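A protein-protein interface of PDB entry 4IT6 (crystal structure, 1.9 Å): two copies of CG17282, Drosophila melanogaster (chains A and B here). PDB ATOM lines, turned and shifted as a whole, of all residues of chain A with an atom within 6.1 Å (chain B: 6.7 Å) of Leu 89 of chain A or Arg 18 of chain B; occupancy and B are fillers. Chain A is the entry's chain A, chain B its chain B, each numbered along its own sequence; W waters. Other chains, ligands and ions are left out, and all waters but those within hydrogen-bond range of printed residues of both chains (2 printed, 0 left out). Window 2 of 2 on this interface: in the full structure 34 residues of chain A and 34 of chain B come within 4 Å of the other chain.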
ATOM      1  N   MET A  76      38.920  13.954   3.326  1.00  0.00           N
ATOM      2  CA  MET A  76      38.353  15.045   2.547  1.00  0.00           C
ATOM      3  C   MET A  76      38.930  15.077   1.135  1.00  0.00           C
ATOM      4  O   MET A  76      40.123  14.852   0.936  1.00  0.00           O
ATOM      5  CB  MET A  76      38.579  16.384   3.252  1.00  0.00           C
ATOM      6  CG  MET A  76      37.992  16.448   4.650  1.00  0.00           C
ATOM      7  SD  MET A  76      36.040  16.411   4.661  1.00  0.00           S
ATOM      8  CE  MET A  76      35.748  16.510   6.582  1.00  0.00           C
ATOM      9  N   ASP A  84      27.729  12.832  -0.896  1.00  0.00           N
ATOM     10  CA  ASP A  84      28.934  12.728  -0.091  1.00  0.00           C
ATOM     11  C   ASP A  84      29.731  14.018  -0.111  1.00  0.00           C
ATOM     12  O   ASP A  84      30.316  14.407   0.899  1.00  0.00           O
ATOM     13  CB  ASP A  84      29.789  11.545  -0.500  1.00  0.00           C
ATOM     14  CG  ASP A  84      29.074  10.209  -0.253  1.00  0.00           C
ATOM     15  OD1 ASP A  84      28.107  10.200   0.544  1.00  0.00           O
ATOM     16  OD2 ASP A  84      29.481   9.186  -0.847  1.00  0.00           O
ATOM     17  N   CYS A  85      29.742  14.687  -1.250  1.00  0.00           N
ATOM     18  CA  CYS A  85      30.525  15.915  -1.364  1.00  0.00           C
ATOM     19  C   CYS A  85      29.963  16.989  -0.459  1.00  0.00           C
ATOM     20  O   CYS A  85      30.725  17.737   0.181  1.00  0.00           O
ATOM     21  CB  CYS A  85      30.588  16.391  -2.812  1.00  0.00           C
ATOM     22  SG  CYS A  85      31.632  15.302  -3.849  1.00  0.00           S
ATOM     23  N   TYR A  86      28.635  17.044  -0.379  1.00  0.00           N
ATOM     24  CA  TYR A  86      27.988  18.022   0.478  1.00  0.00           C
ATOM     25  C   TYR A  86      28.171  17.671   1.950  1.00  0.00           C
ATOM     26  O   TYR A  86      28.302  18.555   2.809  1.00  0.00           O
ATOM     27  CB  TYR A  86      26.513  18.201   0.111  1.00  0.00           C
ATOM     28  CG  TYR A  86      26.319  19.107  -1.098  1.00  0.00           C
ATOM     29  CD1 TYR A  86      27.162  20.194  -1.311  1.00  0.00           C
ATOM     30  CD2 TYR A  86      25.314  18.875  -2.019  1.00  0.00           C
ATOM     31  CE1 TYR A  86      27.002  21.026  -2.402  1.00  0.00           C
ATOM     32  CE2 TYR A  86      25.148  19.702  -3.120  1.00  0.00           C
ATOM     33  CZ  TYR A  86      25.991  20.777  -3.302  1.00  0.00           C
ATOM     34  OH  TYR A  86      25.828  21.604  -4.394  1.00  0.00           O
ATOM     35  N   LEU A  87      28.207  16.383   2.244  1.00  0.00           N
ATOM     36  CA  LEU A  87      28.496  15.930   3.602  1.00  0.00           C
ATOM     37  C   LEU A  87      29.936  16.228   4.069  1.00  0.00           C
ATOM     38  O   LEU A  87      30.183  16.428   5.262  1.00  0.00           O
ATOM     39  CB  LEU A  87      28.225  14.441   3.694  1.00  0.00           C
ATOM     40  CG  LEU A  87      28.553  13.818   5.048  1.00  0.00           C
ATOM     41  CD1 LEU A  87      27.465  12.812   5.432  1.00  0.00           C
ATOM     42  CD2 LEU A  87      29.884  13.118   4.940  1.00  0.00           C
ATOM     43  N   GLU A  88      30.894  16.222   3.149  1.00  0.00           N
ATOM     44  CA  GLU A  88      32.220  16.764   3.467  1.00  0.00           C
ATOM     45  C   GLU A  88      32.195  18.240   3.912  1.00  0.00           C
ATOM     46  O   GLU A  88      32.834  18.634   4.906  1.00  0.00           O
ATOM     47  CB  GLU A  88      33.156  16.633   2.261  1.00  0.00           C
ATOM     48  CG  GLU A  88      33.470  15.204   1.858  1.00  0.00           C
ATOM     49  CD  GLU A  88      34.638  15.140   0.885  1.00  0.00           C
ATOM     50  OE1 GLU A  88      35.214  16.207   0.578  1.00  0.00           O
ATOM     51  OE2 GLU A  88      34.988  14.031   0.430  1.00  0.00           O
ATOM     52  N   LEU A  89      31.472  19.061   3.160  1.00  0.00           N
ATOM     53  CA  LEU A  89      31.392  20.486   3.453  1.00  0.00           C
ATOM     54  C   LEU A  89      30.736  20.741   4.806  1.00  0.00           C
ATOM     55  O   LEU A  89      31.158  21.620   5.554  1.00  0.00           O
ATOM     56  CB  LEU A  89      30.633  21.219   2.345  1.00  0.00           C
ATOM     57  CG  LEU A  89      31.369  21.319   1.010  1.00  0.00           C
ATOM     58  CD1 LEU A  89      30.501  21.996  -0.037  1.00  0.00           C
ATOM     59  CD2 LEU A  89      32.687  22.056   1.182  1.00  0.00           C
ATOM     60  N   LEU A  90      29.714  19.955   5.123  1.00  0.00           N
ATOM     61  CA  LEU A  90      29.024  20.085   6.400  1.00  0.00           C
ATOM     62  C   LEU A  90      29.934  19.690   7.559  1.00  0.00           C
ATOM     63  O   LEU A  90      30.031  20.403   8.557  1.00  0.00           O
ATOM     64  CB  LEU A  90      27.756  19.231   6.411  1.00  0.00           C
ATOM     65  CG  LEU A  90      26.536  19.843   5.722  1.00  0.00           C
ATOM     66  CD1 LEU A  90      25.511  18.778   5.384  1.00  0.00           C
ATOM     67  CD2 LEU A  90      25.924  20.933   6.584  1.00  0.00           C
ATOM     68  N   LEU A  91      30.599  18.549   7.420  1.00  0.00           N
ATOM     69  CA  LEU A  91      31.481  18.053   8.465  1.00  0.00           C
ATOM     70  C   LEU A  91      32.618  19.030   8.719  1.00  0.00           C
ATOM     71  O   LEU A  91      33.186  19.068   9.809  1.00  0.00           O
ATOM     72  CB  LEU A  91      32.044  16.685   8.085  1.00  0.00           C
ATOM     73  CG  LEU A  91      31.116  15.498   8.334  1.00  0.00           C
ATOM     74  CD1 LEU A  91      31.716  14.229   7.767  1.00  0.00           C
ATOM     75  CD2 LEU A  91      30.831  15.347   9.817  1.00  0.00           C
ATOM     76  N   GLN A  92      32.947  19.821   7.707  1.00  0.00           N
ATOM     77  CA  GLN A  92      34.013  20.799   7.840  1.00  0.00           C
ATOM     78  C   GLN A  92      33.567  21.995   8.672  1.00  0.00           C
ATOM     79  O   GLN A  92      34.366  22.876   8.978  1.00  0.00           O
ATOM     80  CB  GLN A  92      34.525  21.234   6.467  1.00  0.00           C
ATOM     81  CG  GLN A  92      35.506  20.245   5.857  1.00  0.00           C
ATOM     82  CD  GLN A  92      35.921  20.616   4.449  1.00  0.00           C
ATOM     83  OE1 GLN A  92      35.798  19.819   3.522  1.00  0.00           O
ATOM     84  NE2 GLN A  92      36.412  21.836   4.282  1.00  0.00           N
ATOM     85  N   GLN A  93      32.292  22.020   9.054  1.00  0.00           N
ATOM     86  CA  GLN A  93      31.813  23.056   9.956  1.00  0.00           C
ATOM     87  C   GLN A  93      31.593  22.577  11.407  1.00  0.00           C
ATOM     88  O   GLN A  93      31.100  23.347  12.237  1.00  0.00           O
ATOM     89  CB  GLN A  93      30.528  23.704   9.406  1.00  0.00           C
ATOM     90  CG  GLN A  93      30.522  23.890   7.879  1.00  0.00           C
ATOM     91  CD  GLN A  93      31.758  24.636   7.372  1.00  0.00           C
ATOM     92  OE1 GLN A  93      32.266  25.548   8.028  1.00  0.00           O
ATOM     93  NE2 GLN A  93      32.256  24.231   6.215  1.00  0.00           N
ATOM     94  N   ILE A 104      20.524  18.854   3.379  1.00  0.00           N
ATOM     95  CA  ILE A 104      20.932  19.292   2.066  1.00  0.00           C
ATOM     96  C   ILE A 104      19.640  19.514   1.311  1.00  0.00           C
ATOM     97  O   ILE A 104      18.869  18.570   1.140  1.00  0.00           O
ATOM     98  CB  ILE A 104      21.706  18.167   1.314  1.00  0.00           C
ATOM     99  CG1 ILE A 104      23.005  17.814   2.044  1.00  0.00           C
ATOM    100  CG2 ILE A 104      21.977  18.574  -0.125  1.00  0.00           C
ATOM    101  CD1 ILE A 104      23.674  16.496   1.512  1.00  0.00           C
ATOM    102  N   THR A 105      19.406  20.740   0.846  1.00  0.00           N
ATOM    103  CA  THR A 105      18.244  21.026   0.000  1.00  0.00           C
ATOM    104  C   THR A 105      18.684  21.170  -1.465  1.00  0.00           C
ATOM    105  O   THR A 105      19.578  21.945  -1.777  1.00  0.00           O
ATOM    106  CB  THR A 105      17.534  22.311   0.437  1.00  0.00           C
ATOM    107  OG1 THR A 105      17.129  22.194   1.803  1.00  0.00           O
ATOM    108  CG2 THR A 105      16.295  22.551  -0.429  1.00  0.00           C
ATOM    109  N   TRP B  13      23.967  27.009  11.421  1.00  0.00           N
ATOM    110  CA  TRP B  13      24.874  27.448  10.367  1.00  0.00           C
ATOM    111  C   TRP B  13      24.194  27.195   9.036  1.00  0.00           C
ATOM    112  O   TRP B  13      23.510  26.185   8.870  1.00  0.00           O
ATOM    113  CB  TRP B  13      26.179  26.660  10.427  1.00  0.00           C
ATOM    114  CG  TRP B  13      27.105  26.976   9.288  1.00  0.00           C
ATOM    115  CD1 TRP B  13      28.042  27.974   9.244  1.00  0.00           C
ATOM    116  CD2 TRP B  13      27.179  26.303   8.026  1.00  0.00           C
ATOM    117  NE1 TRP B  13      28.703  27.953   8.038  1.00  0.00           N
ATOM    118  CE2 TRP B  13      28.191  26.934   7.270  1.00  0.00           C
ATOM    119  CE3 TRP B  13      26.508  25.207   7.470  1.00  0.00           C
ATOM    120  CZ2 TRP B  13      28.529  26.524   5.978  1.00  0.00           C
ATOM    121  CZ3 TRP B  13      26.855  24.790   6.195  1.00  0.00           C
ATOM    122  CH2 TRP B  13      27.854  25.450   5.457  1.00  0.00           C
ATOM    123  N   ASP B  15      24.598  27.547   4.551  1.00  0.00           N
ATOM    124  CA  ASP B  15      25.111  28.015   3.275  1.00  0.00           C
ATOM    125  C   ASP B  15      23.884  28.026   2.398  1.00  0.00           C
ATOM    126  O   ASP B  15      23.533  27.002   1.785  1.00  0.00           O
ATOM    127  CB  ASP B  15      26.177  27.087   2.687  1.00  0.00           C
ATOM    128  CG  ASP B  15      26.652  27.542   1.305  1.00  0.00           C
ATOM    129  OD1 ASP B  15      25.942  28.351   0.678  1.00  0.00           O
ATOM    130  OD2 ASP B  15      27.721  27.083   0.833  1.00  0.00           O
ATOM    131  N   LYS B  16      23.224  29.181   2.377  1.00  0.00           N
ATOM    132  CA  LYS B  16      21.974  29.375   1.654  1.00  0.00           C
ATOM    133  C   LYS B  16      22.111  29.190   0.175  1.00  0.00           C
ATOM    134  O   LYS B  16      21.184  28.721  -0.475  1.00  0.00           O
ATOM    135  CB  LYS B  16      21.390  30.750   1.939  1.00  0.00           C
ATOM    136  CG  LYS B  16      20.641  30.741   3.231  1.00  0.00           C
ATOM    137  CD  LYS B  16      19.316  31.490   3.151  1.00  0.00           C
ATOM    138  CE  LYS B  16      18.247  30.829   4.026  1.00  0.00           C
ATOM    139  NZ  LYS B  16      18.818  30.449   5.367  1.00  0.00           N
ATOM    140  N   ASN B  17      23.281  29.521  -0.352  1.00  0.00           N
ATOM    141  CA  ASN B  17      23.507  29.425  -1.783  1.00  0.00           C
ATOM    142  C   ASN B  17      23.529  27.978  -2.270  1.00  0.00           C
ATOM    143  O   ASN B  17      23.125  27.677  -3.392  1.00  0.00           O
ATOM    144  CB  ASN B  17      24.797  30.148  -2.140  1.00  0.00           C
ATOM    145  CG  ASN B  17      24.651  31.649  -2.049  1.00  0.00           C
ATOM    146  OD1 ASN B  17      23.771  32.227  -2.681  1.00  0.00           O
ATOM    147  ND2 ASN B  17      25.498  32.282  -1.254  1.00  0.00           N
ATOM    148  N   ARG B  18      23.975  27.075  -1.413  1.00  0.00           N
ATOM    149  CA  ARG B  18      24.027  25.687  -1.798  1.00  0.00           C
ATOM    150  C   ARG B  18      23.090  24.774  -1.023  1.00  0.00           C
ATOM    151  O   ARG B  18      23.232  23.562  -1.084  1.00  0.00           O
ATOM    152  CB  ARG B  18      25.457  25.178  -1.739  1.00  0.00           C
ATOM    153  CG  ARG B  18      26.289  25.750  -2.860  1.00  0.00           C
ATOM    154  CD  ARG B  18      27.655  25.166  -2.831  1.00  0.00           C
ATOM    155  NE  ARG B  18      28.352  25.590  -1.630  1.00  0.00           N
ATOM    156  CZ  ARG B  18      29.621  25.309  -1.380  1.00  0.00           C
ATOM    157  NH1 ARG B  18      30.320  24.593  -2.256  1.00  0.00           N
ATOM    158  NH2 ARG B  18      30.180  25.747  -0.263  1.00  0.00           N
ATOM    159  N   GLY B  19      22.116  25.358  -0.334  1.00  0.00           N
ATOM    160  CA  GLY B  19      21.107  24.572   0.364  1.00  0.00           C
ATOM    161  C   GLY B  19      21.611  23.716   1.523  1.00  0.00           C
ATOM    162  O   GLY B  19      21.069  22.632   1.771  1.00  0.00           O
ATOM    163  N   LEU B  20      22.622  24.191   2.252  1.00  0.00           N
ATOM    164  CA  LEU B  20      23.173  23.399   3.337  1.00  0.00           C
ATOM    165  C   LEU B  20      22.815  24.044   4.662  1.00  0.00           C
ATOM    166  O   LEU B  20      22.956  25.265   4.816  1.00  0.00           O
ATOM    167  CB  LEU B  20      24.691  23.280   3.217  1.00  0.00           C
ATOM    168  CG  LEU B  20      25.219  22.710   1.902  1.00  0.00           C
ATOM    169  CD1 LEU B  20      26.749  22.807   1.881  1.00  0.00           C
ATOM    170  CD2 LEU B  20      24.771  21.272   1.721  1.00  0.00           C
HETATM  171  O   HOH W   1      22.352  21.169  -2.303  1.00  0.00           O
HETATM  172  O   HOH W   2      19.011  22.553   3.828  1.00  0.00           O
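No position is printed for both chains.
O of Gly 19 of chain B lies within hydrogen-bond range of N of Thr 105 of chain A (2.7 Å).
CD2 of Leu 20 of chain B touches CG of Tyr 86 of chain A (3.9 Å).
Arg 18 of chain B touches Leu 89 of chain A.
Leu 90 of chain A touches Trp 13 of chain B.
Trp 13 of chain B touches Gln 93 of chain A (CZ2 to CG, 3.8 Å).
O of Gly 19 of chain B touches CA of Ile 104 of chain A, 3.4 Å away.
CG1 of Ile 104 of chain A touches CD2 of Leu 20 of chain B, 3.9 Å away.
O of Leu 89 of chain A is in hydrogen-bond range of NE2 of Gln 93 of chain A (2.9 Å).
The guanidinium group (NE) of Arg 18 of chain B is in salt-bridge range of the side-chain carboxylate (OD2) of Asp 15 of chain B (2.9 Å).
The backbone NH (N) of Asp 15 of chain B lies within hydrogen-bond range of the backbone carbonyl oxygen (O) of Leu 20 of chain B, at 2.8 Å.
Printed residues of chain A that touch a printed residue of chain B: Tyr 86, Leu 89, Leu 90, Gln 93, Ile 104 and Thr 105.
Hydrophobic or aromatic side chains of chain A that line the printed part of chain B: Tyr 86, Leu 89, Leu 90 and Ile 104.
Of the 7 printed residues of chain B, 4 touch a printed residue of chain A.
Among the printed residues, 7 pairs touch across the chains.
Among the printed residues, no Asp or Glu carboxylate lies within 4 Å of a Lys or Arg side-chain nitrogen of the other chain.
Water W2 bridges OG1 of Thr 105 of chain A (2.8 Å) and O of Gly 19 of chain B (2.9 Å).
Water W1 bridges O of Arg 18 of chain B and O of Thr 105 of chain A.
Of the printed residues of chain B, Tyr 86 of chain A touches Leu 20 (3.9 Å).
Of the printed residues of chain B, Leu 90 of chain A touches Trp 13.
Of the printed residues of chain B, Ile 104 of chain A touches Gly 19 (3.4 Å) and Leu 20 (3.9 Å).
The nearest residue of chain B that does not touch Leu 89 of chain A is Leu 20 of chain B (4.2 Å).
The nearest residue of chain A that does not touch Arg 18 of chain B is Thr 105 of chain A (4.1 Å).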
